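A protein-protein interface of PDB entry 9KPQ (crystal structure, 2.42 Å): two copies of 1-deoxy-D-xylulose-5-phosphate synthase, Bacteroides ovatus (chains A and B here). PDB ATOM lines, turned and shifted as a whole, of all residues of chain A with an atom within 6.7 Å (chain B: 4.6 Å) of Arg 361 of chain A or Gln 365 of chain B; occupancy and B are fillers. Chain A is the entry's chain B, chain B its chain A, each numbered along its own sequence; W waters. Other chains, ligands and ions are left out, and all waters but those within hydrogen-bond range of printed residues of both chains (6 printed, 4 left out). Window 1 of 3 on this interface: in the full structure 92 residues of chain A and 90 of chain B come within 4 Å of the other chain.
N of Leu 370 of chain B sits at hydrogen-bond distance from O of Gln 365 of chain B, 2.8 Å away. OG1 of Thr 357 of chain A lies within hydrogen-bond range of NE2 of His 117 of chain A (2.8 Å). The guanidinium group (NH2) of Arg 361 of chain A sits at hydrogen-bond distance from the backbone carbonyl oxygen (O) of Thr 118 of chain A (2.8 Å). The side-chain carboxylate (OE1) of Glu 154 of chain A is in salt-bridge range of the guanidinium group (NH2) of Arg 361 of chain A (3.9 Å).
Arg 361 of chain A touches Asp 364 of chain B, and with the chains exchanged Asp 364 of chain A touches Arg 361 of chain B. Arg 361 of chain A touches Gln 365 of chain B, and with the chains exchanged Gln 365 of chain A touches Arg 361 of chain B. Positions printed for both chains: 334, 361, 362, 363, 364 and 365.
Water W2 lies within hydrogen-bond range of the side-chain carboxylate (OD1) of Asp 369 of chain B and the side-chain hydroxyl (OG1) of Thr 120 of chain A. Water W1 lies within hydrogen-bond range of the side-chain hydroxyl of Ser 367 of chain B (2.6 Å), the side-chain amide oxygen of Gln 360 of chain A (3.1 Å) and the side-chain amide nitrogen of Gln 368 of chain B (3.2 Å). Water W3 lies within hydrogen-bond range of the side-chain amide oxygen of Gln 368 of chain B (2.9 Å), the backbone NH of Gly 116 of chain A (2.9 Å) and the backbone NH of His 117 of chain A (3.0 Å). Water W5 lies within hydrogen-bond range of OD2 of Asp 364 of chain A and NH2 of Arg 361 of chain B. Water W4 bridges OE2 of Glu 334 of chain A and OE2 of Glu 334 of chain B. Water W6 lies within hydrogen-bond range of OE2 of Glu 334 of chain B (3.1 Å), O of Arg 361 of chain B (3.2 Å) and NE2 of Gln 365 of chain A (3.2 Å).
Ser 119 of chain A touches none of the printed residues of chain B. Of the printed residues of chain B, Glu 154 of chain A touches Gln 365 (2.7 Å) and Asp 369 (2.7 Å). Printed residues of chain B within 4 Å of Gln 360 of chain A: Tyr 363 and Asp 364. Of the printed residues of chain B, Arg 361 of chain A touches Asp 364 (2.9 Å) and Gln 365 (3.3 Å). Of the printed residues of chain B, Gln 365 of chain A touches Arg 361 (3.3 Å). Of chain A, only Glu 154 (2.7 Å) and Arg 361 (3.3 Å) come within 4 Å of Gln 365 of chain B. Of the printed residues of chain A, Gln 368 of chain B touches His 117.
Along chain B the printed residues that touch a printed residue of chain A span positions 361 to 369. Of the 22 printed residues of chain A, 8 touch a printed residue of chain B. Printed residues of chain A that touch a printed residue of chain B: His 117, Thr 120, Glu 154, Gln 360, Arg 361, Asp 364, Gln 365 and Leu 402. Among the printed residues, 12 pairs touch across the chains.
The guanidinium group (NE) of Arg 361 of chain B lies within salt-bridge range of the side-chain carboxylate (OD2) of Asp 364 of chain A (2.4 Å). NE2 of Gln 365 of chain A lies close to NE of Arg 361 of chain B, 3.4 Å away. The side-chain carboxylate (OD2) of Asp 364 of chain B sits at hydrogen-bond distance from a ring nitrogen (ND1) of His 117 of chain A (2.7 Å). OD1 of Asp 364 of chain B lies close to OE1 of Gln 360 of chain A (2.8 Å). OD2 of Asp 364 of chain B is in salt-bridge range of NE of Arg 361 of chain A, 2.9 Å away. The side-chain amide nitrogen (NE2) of Gln 365 of chain B sits at hydrogen-bond distance from the side-chain carboxylate (OE1) of Glu 154 of chain A (2.7 Å). The guanidinium group (NE) of Arg 361 of chain A sits close to the side-chain amide nitrogen (NE2) of Gln 365 of chain B (3.3 Å). A ring nitrogen (ND1) of His 117 of chain A sits close to the side-chain amide oxygen (OE1) of Gln 368 of chain B, at 3.4 Å. OD2 of Asp 369 of chain B lies close to OE2 of Glu 154 of chain A (2.7 Å).
Among the printed residues, merely in contact across the chains: Thr 120 of chain A with Asp 369 of chain B, Gln 360 of chain A with Tyr 363 of chain B and Leu 402 of chain A with Tyr 363 of chain B.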
ATOM      1  N   GLY A 116      -6.113  -8.766 -26.334  1.00  0.00           N
ATOM      2  CA  GLY A 116      -5.633  -9.866 -27.143  1.00  0.00           C
ATOM      3  C   GLY A 116      -6.230 -11.207 -26.705  1.00  0.00           C
ATOM      4  O   GLY A 116      -6.563 -12.038 -27.554  1.00  0.00           O
ATOM      5  N   HIS A 117      -6.353 -11.446 -25.401  1.00  0.00           N
ATOM      6  CA  HIS A 117      -6.832 -12.765 -24.946  1.00  0.00           C
ATOM      7  C   HIS A 117      -8.388 -12.869 -25.095  1.00  0.00           C
ATOM      8  O   HIS A 117      -9.056 -11.889 -25.464  1.00  0.00           O
ATOM      9  CB  HIS A 117      -6.373 -13.036 -23.509  1.00  0.00           C
ATOM     10  CG  HIS A 117      -4.928 -13.420 -23.403  1.00  0.00           C
ATOM     11  ND1 HIS A 117      -4.374 -13.933 -22.249  1.00  0.00           N
ATOM     12  CD2 HIS A 117      -3.921 -13.365 -24.311  1.00  0.00           C
ATOM     13  CE1 HIS A 117      -3.094 -14.193 -22.458  1.00  0.00           C
ATOM     14  NE2 HIS A 117      -2.792 -13.850 -23.697  1.00  0.00           N
ATOM     15  N   THR A 118      -8.956 -14.050 -24.865  1.00  0.00           N
ATOM     16  CA  THR A 118     -10.385 -14.270 -25.164  1.00  0.00           C
ATOM     17  C   THR A 118     -11.331 -14.009 -23.978  1.00  0.00           C
ATOM     18  O   THR A 118     -10.921 -14.062 -22.807  1.00  0.00           O
ATOM     19  CB  THR A 118     -10.628 -15.714 -25.645  1.00  0.00           C
ATOM     20  OG1 THR A 118     -10.132 -16.638 -24.661  1.00  0.00           O
ATOM     21  CG2 THR A 118      -9.904 -15.953 -26.957  1.00  0.00           C
ATOM     22  N   SER A 119     -12.586 -13.792 -24.296  1.00  0.00           N
ATOM     23  CA  SER A 119     -13.675 -13.621 -23.343  1.00  0.00           C
ATOM     24  C   SER A 119     -13.533 -12.524 -22.276  1.00  0.00           C
ATOM     25  O   SER A 119     -13.867 -12.771 -21.205  1.00  0.00           O
ATOM     26  CB  SER A 119     -14.002 -14.952 -22.667  1.00  0.00           C
ATOM     27  OG  SER A 119     -13.438 -16.037 -23.257  1.00  0.00           O
ATOM     28  N   THR A 120     -13.014 -11.343 -22.599  1.00  0.00           N
ATOM     29  CA  THR A 120     -12.830 -10.298 -21.588  1.00  0.00           C
ATOM     30  C   THR A 120     -13.603  -9.038 -21.897  1.00  0.00           C
ATOM     31  O   THR A 120     -13.726  -8.153 -21.034  1.00  0.00           O
ATOM     32  CB  THR A 120     -11.363  -9.881 -21.422  1.00  0.00           C
ATOM     33  OG1 THR A 120     -11.039  -8.924 -22.439  1.00  0.00           O
ATOM     34  CG2 THR A 120     -10.434 -11.072 -21.520  1.00  0.00           C
ATOM     35  N   GLY A 152     -15.601 -19.374 -22.930  1.00  0.00           N
ATOM     36  CA  GLY A 152     -14.671 -19.078 -21.856  1.00  0.00           C
ATOM     37  C   GLY A 152     -15.388 -18.574 -20.625  1.00  0.00           C
ATOM     38  O   GLY A 152     -16.280 -17.741 -20.745  1.00  0.00           O
ATOM     39  N   GLY A 153     -14.998 -19.055 -19.450  1.00  0.00           N
ATOM     40  CA  GLY A 153     -15.700 -18.731 -18.216  1.00  0.00           C
ATOM     41  C   GLY A 153     -15.760 -17.257 -17.820  1.00  0.00           C
ATOM     42  O   GLY A 153     -16.721 -16.823 -17.181  1.00  0.00           O
ATOM     43  N   GLU A 154     -14.761 -16.465 -18.209  1.00  0.00           N
ATOM     44  CA  GLU A 154     -14.823 -15.019 -17.947  1.00  0.00           C
ATOM     45  C   GLU A 154     -16.028 -14.377 -18.655  1.00  0.00           C
ATOM     46  O   GLU A 154     -16.627 -13.437 -18.139  1.00  0.00           O
ATOM     47  CB  GLU A 154     -13.539 -14.331 -18.387  1.00  0.00           C
ATOM     48  CG  GLU A 154     -13.338 -12.968 -17.759  1.00  0.00           C
ATOM     49  CD  GLU A 154     -11.991 -12.335 -18.105  1.00  0.00           C
ATOM     50  OE1 GLU A 154     -10.967 -13.068 -18.194  1.00  0.00           O
ATOM     51  OE2 GLU A 154     -11.963 -11.093 -18.272  1.00  0.00           O
ATOM     52  N   ILE A 331     -12.579 -22.549 -25.515  1.00  0.00           N
ATOM     53  CA  ILE A 331     -11.546 -21.647 -25.029  1.00  0.00           C
ATOM     54  C   ILE A 331     -11.600 -21.609 -23.493  1.00  0.00           C
ATOM     55  O   ILE A 331     -11.878 -20.567 -22.872  1.00  0.00           O
ATOM     56  CB  ILE A 331     -11.706 -20.271 -25.650  1.00  0.00           C
ATOM     57  CG1 ILE A 331     -11.442 -20.375 -27.156  1.00  0.00           C
ATOM     58  CG2 ILE A 331     -10.689 -19.326 -25.048  1.00  0.00           C
ATOM     59  CD1 ILE A 331     -11.820 -19.144 -27.927  1.00  0.00           C
ATOM     60  N   GLU A 333      -9.230 -22.798 -20.817  1.00  0.00           N
ATOM     61  CA  GLU A 333      -7.938 -23.205 -20.278  1.00  0.00           C
ATOM     62  C   GLU A 333      -8.043 -23.714 -18.844  1.00  0.00           C
ATOM     63  O   GLU A 333      -7.404 -24.714 -18.474  1.00  0.00           O
ATOM     64  CB  GLU A 333      -6.966 -22.036 -20.357  1.00  0.00           C
ATOM     65  CG  GLU A 333      -6.531 -21.719 -21.794  1.00  0.00           C
ATOM     66  CD  GLU A 333      -7.404 -20.663 -22.452  1.00  0.00           C
ATOM     67  OE1 GLU A 333      -8.557 -20.449 -22.012  1.00  0.00           O
ATOM     68  OE2 GLU A 333      -6.928 -20.029 -23.416  1.00  0.00           O
ATOM     69  N   GLU A 334      -8.870 -23.041 -18.046  1.00  0.00           N
ATOM     70  CA  GLU A 334      -9.068 -23.427 -16.660  1.00  0.00           C
ATOM     71  C   GLU A 334      -9.627 -24.835 -16.580  1.00  0.00           C
ATOM     72  O   GLU A 334      -9.126 -25.658 -15.828  1.00  0.00           O
ATOM     73  CB  GLU A 334     -10.010 -22.456 -15.940  1.00  0.00           C
ATOM     74  CG  GLU A 334      -9.589 -20.982 -16.006  1.00  0.00           C
ATOM     75  CD  GLU A 334     -10.146 -20.269 -17.228  1.00  0.00           C
ATOM     76  OE1 GLU A 334     -10.228 -20.905 -18.308  1.00  0.00           O
ATOM     77  OE2 GLU A 334     -10.516 -19.077 -17.105  1.00  0.00           O
ATOM     78  N   SER A 356       2.151 -20.755 -24.098  1.00  0.00           N
ATOM     79  CA  SER A 356       2.628 -20.091 -22.917  1.00  0.00           C
ATOM     80  C   SER A 356       1.729 -18.915 -22.492  1.00  0.00           C
ATOM     81  O   SER A 356       1.297 -18.855 -21.338  1.00  0.00           O
ATOM     82  CB  SER A 356       4.055 -19.600 -23.170  1.00  0.00           C
ATOM     83  OG  SER A 356       4.415 -18.604 -22.237  1.00  0.00           O
ATOM     84  N   THR A 357       1.445 -17.992 -23.415  1.00  0.00           N
ATOM     85  CA  THR A 357       0.705 -16.785 -23.081  1.00  0.00           C
ATOM     86  C   THR A 357      -0.717 -17.131 -22.577  1.00  0.00           C
ATOM     87  O   THR A 357      -1.251 -16.415 -21.713  1.00  0.00           O
ATOM     88  CB  THR A 357       0.629 -15.791 -24.302  1.00  0.00           C
ATOM     89  OG1 THR A 357      -0.150 -14.629 -23.964  1.00  0.00           O
ATOM     90  CG2 THR A 357       0.000 -16.458 -25.544  1.00  0.00           C
ATOM     91  N   PHE A 358      -1.316 -18.226 -23.077  1.00  0.00           N
ATOM     92  CA  PHE A 358      -2.693 -18.583 -22.689  1.00  0.00           C
ATOM     93  C   PHE A 358      -2.771 -19.409 -21.412  1.00  0.00           C
ATOM     94  O   PHE A 358      -3.792 -19.368 -20.715  1.00  0.00           O
ATOM     95  CB  PHE A 358      -3.406 -19.350 -23.799  1.00  0.00           C
ATOM     96  CG  PHE A 358      -3.492 -18.607 -25.092  1.00  0.00           C
ATOM     97  CD1 PHE A 358      -3.597 -17.228 -25.109  1.00  0.00           C
ATOM     98  CD2 PHE A 358      -3.445 -19.286 -26.300  1.00  0.00           C
ATOM     99  CE1 PHE A 358      -3.656 -16.532 -26.317  1.00  0.00           C
ATOM    100  CE2 PHE A 358      -3.508 -18.602 -27.506  1.00  0.00           C
ATOM    101  CZ  PHE A 358      -3.614 -17.227 -27.520  1.00  0.00           C
ATOM    102  N   ILE A 359      -1.731 -20.180 -21.100  1.00  0.00           N
ATOM    103  CA  ILE A 359      -1.768 -21.000 -19.880  1.00  0.00           C
ATOM    104  C   ILE A 359      -1.795 -20.110 -18.615  1.00  0.00           C
ATOM    105  O   ILE A 359      -2.083 -20.583 -17.507  1.00  0.00           O
ATOM    106  CB  ILE A 359      -0.596 -22.022 -19.845  1.00  0.00           C
ATOM    107  CG1 ILE A 359      -0.810 -23.037 -18.715  1.00  0.00           C
ATOM    108  CG2 ILE A 359       0.733 -21.335 -19.663  1.00  0.00           C
ATOM    109  CD1 ILE A 359      -2.027 -23.948 -18.927  1.00  0.00           C
ATOM    110  N   GLN A 360      -1.516 -18.820 -18.807  1.00  0.00           N
ATOM    111  CA  GLN A 360      -1.608 -17.810 -17.756  1.00  0.00           C
ATOM    112  C   GLN A 360      -2.993 -17.779 -17.087  1.00  0.00           C
ATOM    113  O   GLN A 360      -3.136 -17.209 -16.007  1.00  0.00           O
ATOM    114  CB  GLN A 360      -1.297 -16.412 -18.314  1.00  0.00           C
ATOM    115  CG  GLN A 360       0.152 -16.102 -18.676  1.00  0.00           C
ATOM    116  CD  GLN A 360       0.298 -14.715 -19.346  1.00  0.00           C
ATOM    117  OE1 GLN A 360      -0.597 -13.850 -19.233  1.00  0.00           O
ATOM    118  NE2 GLN A 360       1.414 -14.513 -20.065  1.00  0.00           N
ATOM    119  N   ARG A 361      -4.014 -18.329 -17.751  1.00  0.00           N
ATOM    120  CA  ARG A 361      -5.375 -18.339 -17.210  1.00  0.00           C
ATOM    121  C   ARG A 361      -5.583 -19.334 -16.074  1.00  0.00           C
ATOM    122  O   ARG A 361      -6.579 -19.241 -15.358  1.00  0.00           O
ATOM    123  CB  ARG A 361      -6.392 -18.640 -18.303  1.00  0.00           C
ATOM    124  CG  ARG A 361      -6.716 -17.460 -19.199  1.00  0.00           C
ATOM    125  CD  ARG A 361      -7.898 -16.637 -18.693  1.00  0.00           C
ATOM    126  NE  ARG A 361      -7.984 -15.399 -19.454  1.00  0.00           N
ATOM    127  CZ  ARG A 361      -8.772 -15.208 -20.499  1.00  0.00           C
ATOM    128  NH1 ARG A 361      -9.622 -16.135 -20.900  1.00  0.00           N
ATOM    129  NH2 ARG A 361      -8.664 -14.080 -21.194  1.00  0.00           N
ATOM    130  N   SER A 362      -4.672 -20.289 -15.905  1.00  0.00           N
ATOM    131  CA  SER A 362      -4.986 -21.455 -15.092  1.00  0.00           C
ATOM    132  C   SER A 362      -4.106 -21.635 -13.884  1.00  0.00           C
ATOM    133  O   SER A 362      -3.802 -22.773 -13.511  1.00  0.00           O
ATOM    134  CB  SER A 362      -4.895 -22.724 -15.943  1.00  0.00           C
ATOM    135  OG  SER A 362      -5.479 -22.500 -17.208  1.00  0.00           O
ATOM    136  N   TYR A 363      -3.695 -20.552 -13.245  1.00  0.00           N
ATOM    137  CA  TYR A 363      -2.778 -20.735 -12.140  1.00  0.00           C
ATOM    138  C   TYR A 363      -3.452 -21.542 -11.011  1.00  0.00           C
ATOM    139  O   TYR A 363      -2.874 -22.511 -10.512  1.00  0.00           O
ATOM    140  CB  TYR A 363      -2.231 -19.393 -11.626  1.00  0.00           C
ATOM    141  CG  TYR A 363      -1.324 -19.568 -10.424  1.00  0.00           C
ATOM    142  CD1 TYR A 363      -1.865 -19.741  -9.156  1.00  0.00           C
ATOM    143  CD2 TYR A 363       0.070 -19.557 -10.547  1.00  0.00           C
ATOM    144  CE1 TYR A 363      -1.084 -19.895  -8.066  1.00  0.00           C
ATOM    145  CE2 TYR A 363       0.881 -19.712  -9.421  1.00  0.00           C
ATOM    146  CZ  TYR A 363       0.279 -19.882  -8.186  1.00  0.00           C
ATOM    147  OH  TYR A 363       1.004 -20.045  -7.029  1.00  0.00           O
ATOM    148  N   ASP A 364      -4.652 -21.146 -10.609  1.00  0.00           N
ATOM    149  CA  ASP A 364      -5.315 -21.800  -9.474  1.00  0.00           C
ATOM    150  C   ASP A 364      -5.670 -23.254  -9.814  1.00  0.00           C
ATOM    151  O   ASP A 364      -5.723 -24.130  -8.941  1.00  0.00           O
ATOM    152  CB  ASP A 364      -6.585 -21.036  -9.053  1.00  0.00           C
ATOM    153  CG  ASP A 364      -7.086 -21.449  -7.680  1.00  0.00           C
ATOM    154  OD1 ASP A 364      -6.289 -21.438  -6.727  1.00  0.00           O
ATOM    155  OD2 ASP A 364      -8.284 -21.777  -7.531  1.00  0.00           O
ATOM    156  N   GLN A 365      -5.936 -23.513 -11.086  1.00  0.00           N
ATOM    157  CA  GLN A 365      -6.311 -24.863 -11.472  1.00  0.00           C
ATOM    158  C   GLN A 365      -5.057 -25.747 -11.481  1.00  0.00           C
ATOM    159  O   GLN A 365      -5.082 -26.884 -10.996  1.00  0.00           O
ATOM    160  CB  GLN A 365      -7.053 -24.862 -12.824  1.00  0.00           C
ATOM    161  CG  GLN A 365      -8.513 -24.334 -12.721  1.00  0.00           C
ATOM    162  CD  GLN A 365      -8.557 -22.811 -12.741  1.00  0.00           C
ATOM    163  OE1 GLN A 365      -7.626 -22.183 -13.255  1.00  0.00           O
ATOM    164  NE2 GLN A 365      -9.608 -22.210 -12.167  1.00  0.00           N
ATOM    165  N   LEU A 402       5.098 -18.330 -13.774  1.00  0.00           N
ATOM    166  CA  LEU A 402       3.737 -18.757 -13.506  1.00  0.00           C
ATOM    167  C   LEU A 402       3.681 -20.173 -12.901  1.00  0.00           C
ATOM    168  O   LEU A 402       2.966 -20.393 -11.908  1.00  0.00           O
ATOM    169  CB  LEU A 402       2.920 -18.701 -14.793  1.00  0.00           C
ATOM    170  CG  LEU A 402       1.536 -19.335 -14.777  1.00  0.00           C
ATOM    171  CD1 LEU A 402       0.567 -18.434 -14.000  1.00  0.00           C
ATOM    172  CD2 LEU A 402       1.033 -19.614 -16.229  1.00  0.00           C
ATOM    173  N   GLU B 334     -12.158 -13.703 -11.408  1.00  0.00           N
ATOM    174  CA  GLU B 334     -11.624 -13.307 -12.697  1.00  0.00           C
ATOM    175  C   GLU B 334     -12.266 -12.024 -13.154  1.00  0.00           C
ATOM    176  O   GLU B 334     -11.584 -11.048 -13.488  1.00  0.00           O
ATOM    177  CB  GLU B 334     -11.865 -14.408 -13.732  1.00  0.00           C
ATOM    178  CG  GLU B 334     -11.284 -15.768 -13.323  1.00  0.00           C
ATOM    179  CD  GLU B 334     -12.260 -16.607 -12.535  1.00  0.00           C
ATOM    180  OE1 GLU B 334     -13.136 -16.027 -11.853  1.00  0.00           O
ATOM    181  OE2 GLU B 334     -12.162 -17.851 -12.597  1.00  0.00           O
ATOM    182  N   VAL B 337     -11.692  -8.582 -11.360  1.00  0.00           N
ATOM    183  CA  VAL B 337     -10.520  -7.810 -11.737  1.00  0.00           C
ATOM    184  C   VAL B 337     -10.800  -7.024 -13.011  1.00  0.00           C
ATOM    185  O   VAL B 337     -10.484  -5.824 -13.104  1.00  0.00           O
ATOM    186  CB  VAL B 337      -9.266  -8.691 -11.904  1.00  0.00           C
ATOM    187  CG1 VAL B 337      -8.183  -7.912 -12.642  1.00  0.00           C
ATOM    188  CG2 VAL B 337      -8.752  -9.137 -10.550  1.00  0.00           C
ATOM    189  N   ARG B 361      -6.967 -17.215  -8.682  1.00  0.00           N
ATOM    190  CA  ARG B 361      -7.753 -17.493  -9.882  1.00  0.00           C
ATOM    191  C   ARG B 361      -7.525 -16.476 -11.003  1.00  0.00           C
ATOM    192  O   ARG B 361      -7.798 -16.773 -12.170  1.00  0.00           O
ATOM    193  CB  ARG B 361      -9.264 -17.520  -9.564  1.00  0.00           C
ATOM    194  CG  ARG B 361      -9.795 -18.743  -8.819  1.00  0.00           C
ATOM    195  CD  ARG B 361      -9.909 -19.945  -9.722  1.00  0.00           C
ATOM    196  NE  ARG B 361     -10.135 -21.177  -8.971  1.00  0.00           N
ATOM    197  CZ  ARG B 361     -11.333 -21.640  -8.624  1.00  0.00           C
ATOM    198  NH1 ARG B 361     -12.447 -21.023  -8.981  1.00  0.00           N
ATOM    199  NH2 ARG B 361     -11.415 -22.748  -7.905  1.00  0.00           N
ATOM    200  N   SER B 362      -6.976 -15.307 -10.682  1.00  0.00           N
ATOM    201  CA  SER B 362      -7.052 -14.168 -11.600  1.00  0.00           C
ATOM    202  C   SER B 362      -5.723 -13.694 -12.112  1.00  0.00           C
ATOM    203  O   SER B 362      -5.548 -12.500 -12.288  1.00  0.00           O
ATOM    204  CB  SER B 362      -7.745 -12.981 -10.914  1.00  0.00           C
ATOM    205  OG  SER B 362      -8.955 -13.382 -10.270  1.00  0.00           O
ATOM    206  N   TYR B 363      -4.777 -14.599 -12.367  1.00  0.00           N
ATOM    207  CA  TYR B 363      -3.465 -14.137 -12.805  1.00  0.00           C
ATOM    208  C   TYR B 363      -3.545 -13.405 -14.148  1.00  0.00           C
ATOM    209  O   TYR B 363      -3.028 -12.290 -14.274  1.00  0.00           O
ATOM    210  CB  TYR B 363      -2.460 -15.292 -12.913  1.00  0.00           C
ATOM    211  CG  TYR B 363      -1.114 -14.845 -13.473  1.00  0.00           C
ATOM    212  CD1 TYR B 363      -0.901 -14.751 -14.856  1.00  0.00           C
ATOM    213  CD2 TYR B 363      -0.064 -14.503 -12.629  1.00  0.00           C
ATOM    214  CE1 TYR B 363       0.302 -14.332 -15.362  1.00  0.00           C
ATOM    215  CE2 TYR B 363       1.147 -14.093 -13.132  1.00  0.00           C
ATOM    216  CZ  TYR B 363       1.322 -14.014 -14.503  1.00  0.00           C
ATOM    217  OH  TYR B 363       2.517 -13.595 -15.032  1.00  0.00           O
ATOM    218  N   ASP B 364      -4.190 -14.018 -15.139  1.00  0.00           N
ATOM    219  CA  ASP B 364      -4.230 -13.435 -16.490  1.00  0.00           C
ATOM    220  C   ASP B 364      -4.993 -12.116 -16.538  1.00  0.00           C
ATOM    221  O   ASP B 364      -4.688 -11.252 -17.358  1.00  0.00           O
ATOM    222  CB  ASP B 364      -4.871 -14.403 -17.499  1.00  0.00           C
ATOM    223  CG  ASP B 364      -4.545 -14.043 -18.947  1.00  0.00           C
ATOM    224  OD1 ASP B 364      -3.357 -13.808 -19.237  1.00  0.00           O
ATOM    225  OD2 ASP B 364      -5.471 -14.023 -19.802  1.00  0.00           O
ATOM    226  N   GLN B 365      -5.995 -11.987 -15.675  1.00  0.00           N
ATOM    227  CA  GLN B 365      -6.819 -10.784 -15.644  1.00  0.00           C
ATOM    228  C   GLN B 365      -6.036  -9.669 -14.971  1.00  0.00           C
ATOM    229  O   GLN B 365      -6.028  -8.546 -15.469  1.00  0.00           O
ATOM    230  CB  GLN B 365      -8.161 -11.050 -14.934  1.00  0.00           C
ATOM    231  CG  GLN B 365      -9.115 -11.936 -15.746  1.00  0.00           C
ATOM    232  CD  GLN B 365      -8.839 -13.416 -15.562  1.00  0.00           C
ATOM    233  OE1 GLN B 365      -8.398 -13.834 -14.503  1.00  0.00           O
ATOM    234  NE2 GLN B 365      -9.092 -14.216 -16.601  1.00  0.00           N
ATOM    235  N   LEU B 366      -5.355  -9.982 -13.869  1.00  0.00           N
ATOM    236  CA  LEU B 366      -4.414  -9.024 -13.255  1.00  0.00           C
ATOM    237  C   LEU B 366      -3.368  -8.581 -14.302  1.00  0.00           C
ATOM    238  O   LEU B 366      -3.093  -7.390 -14.487  1.00  0.00           O
ATOM    239  CB  LEU B 366      -3.712  -9.625 -12.028  1.00  0.00           C
ATOM    240  CG  LEU B 366      -4.550  -9.998 -10.792  1.00  0.00           C
ATOM    241  CD1 LEU B 366      -3.804 -11.050  -9.918  1.00  0.00           C
ATOM    242  CD2 LEU B 366      -5.000  -8.763  -9.963  1.00  0.00           C
ATOM    243  N   SER B 367      -2.825  -9.542 -15.027  1.00  0.00           N
ATOM    244  CA  SER B 367      -1.770  -9.222 -15.977  1.00  0.00           C
ATOM    245  C   SER B 367      -2.269  -8.439 -17.226  1.00  0.00           C
ATOM    246  O   SER B 367      -1.656  -7.458 -17.645  1.00  0.00           O
ATOM    247  CB  SER B 367      -1.082 -10.519 -16.403  1.00  0.00           C
ATOM    248  OG  SER B 367       0.038 -10.247 -17.203  1.00  0.00           O
ATOM    249  N   GLN B 368      -3.350  -8.919 -17.845  1.00  0.00           N
ATOM    250  CA  GLN B 368      -3.812  -8.402 -19.124  1.00  0.00           C
ATOM    251  C   GLN B 368      -4.911  -7.358 -18.961  1.00  0.00           C
ATOM    252  O   GLN B 368      -4.777  -6.195 -19.398  1.00  0.00           O
ATOM    253  CB  GLN B 368      -4.308  -9.544 -20.012  1.00  0.00           C
ATOM    254  CG  GLN B 368      -3.248 -10.599 -20.372  1.00  0.00           C
ATOM    255  CD  GLN B 368      -2.982 -10.699 -21.879  1.00  0.00           C
ATOM    256  OE1 GLN B 368      -3.907 -10.591 -22.703  1.00  0.00           O
ATOM    257  NE2 GLN B 368      -1.713 -10.925 -22.247  1.00  0.00           N
ATOM    258  N   ASP B 369      -6.016  -7.794 -18.363  1.00  0.00           N
ATOM    259  CA  ASP B 369      -7.147  -6.909 -18.153  1.00  0.00           C
ATOM    260  C   ASP B 369      -6.756  -5.665 -17.344  1.00  0.00           C
ATOM    261  O   ASP B 369      -7.168  -4.554 -17.657  1.00  0.00           O
ATOM    262  CB  ASP B 369      -8.280  -7.677 -17.462  1.00  0.00           C
ATOM    263  CG  ASP B 369      -8.761  -8.873 -18.285  1.00  0.00           C
ATOM    264  OD1 ASP B 369      -8.104  -9.196 -19.308  1.00  0.00           O
ATOM    265  OD2 ASP B 369      -9.789  -9.484 -17.907  1.00  0.00           O
ATOM    266  N   LEU B 370      -5.936  -5.857 -16.322  1.00  0.00           N
ATOM    267  CA  LEU B 370      -5.593  -4.760 -15.426  1.00  0.00           C
ATOM    268  C   LEU B 370      -4.277  -4.097 -15.814  1.00  0.00           C
ATOM    269  O   LEU B 370      -4.259  -2.915 -16.145  1.00  0.00           O
ATOM    270  CB  LEU B 370      -5.517  -5.251 -13.973  1.00  0.00           C
ATOM    271  CG  LEU B 370      -5.181  -4.187 -12.918  1.00  0.00           C
ATOM    272  CD1 LEU B 370      -6.126  -2.981 -13.005  1.00  0.00           C
ATOM    273  CD2 LEU B 370      -5.198  -4.783 -11.506  1.00  0.00           C
HETATM  274  O   HOH W   1       0.224 -10.880 -19.759  1.00  0.00           O
HETATM  275  O   HOH W   2      -8.145  -8.483 -21.677  1.00  0.00           O
HETATM  276  O   HOH W   3      -6.259  -9.135 -23.430  1.00  0.00           O
HETATM  277  O   HOH W   4     -13.090 -18.812 -15.570  1.00  0.00           O
HETATM  278  O   HOH W   5      -8.980 -24.223  -9.030  1.00  0.00           O
HETATM  279  O   HOH W   6      -9.503 -19.212 -13.221  1.00  0.00           O
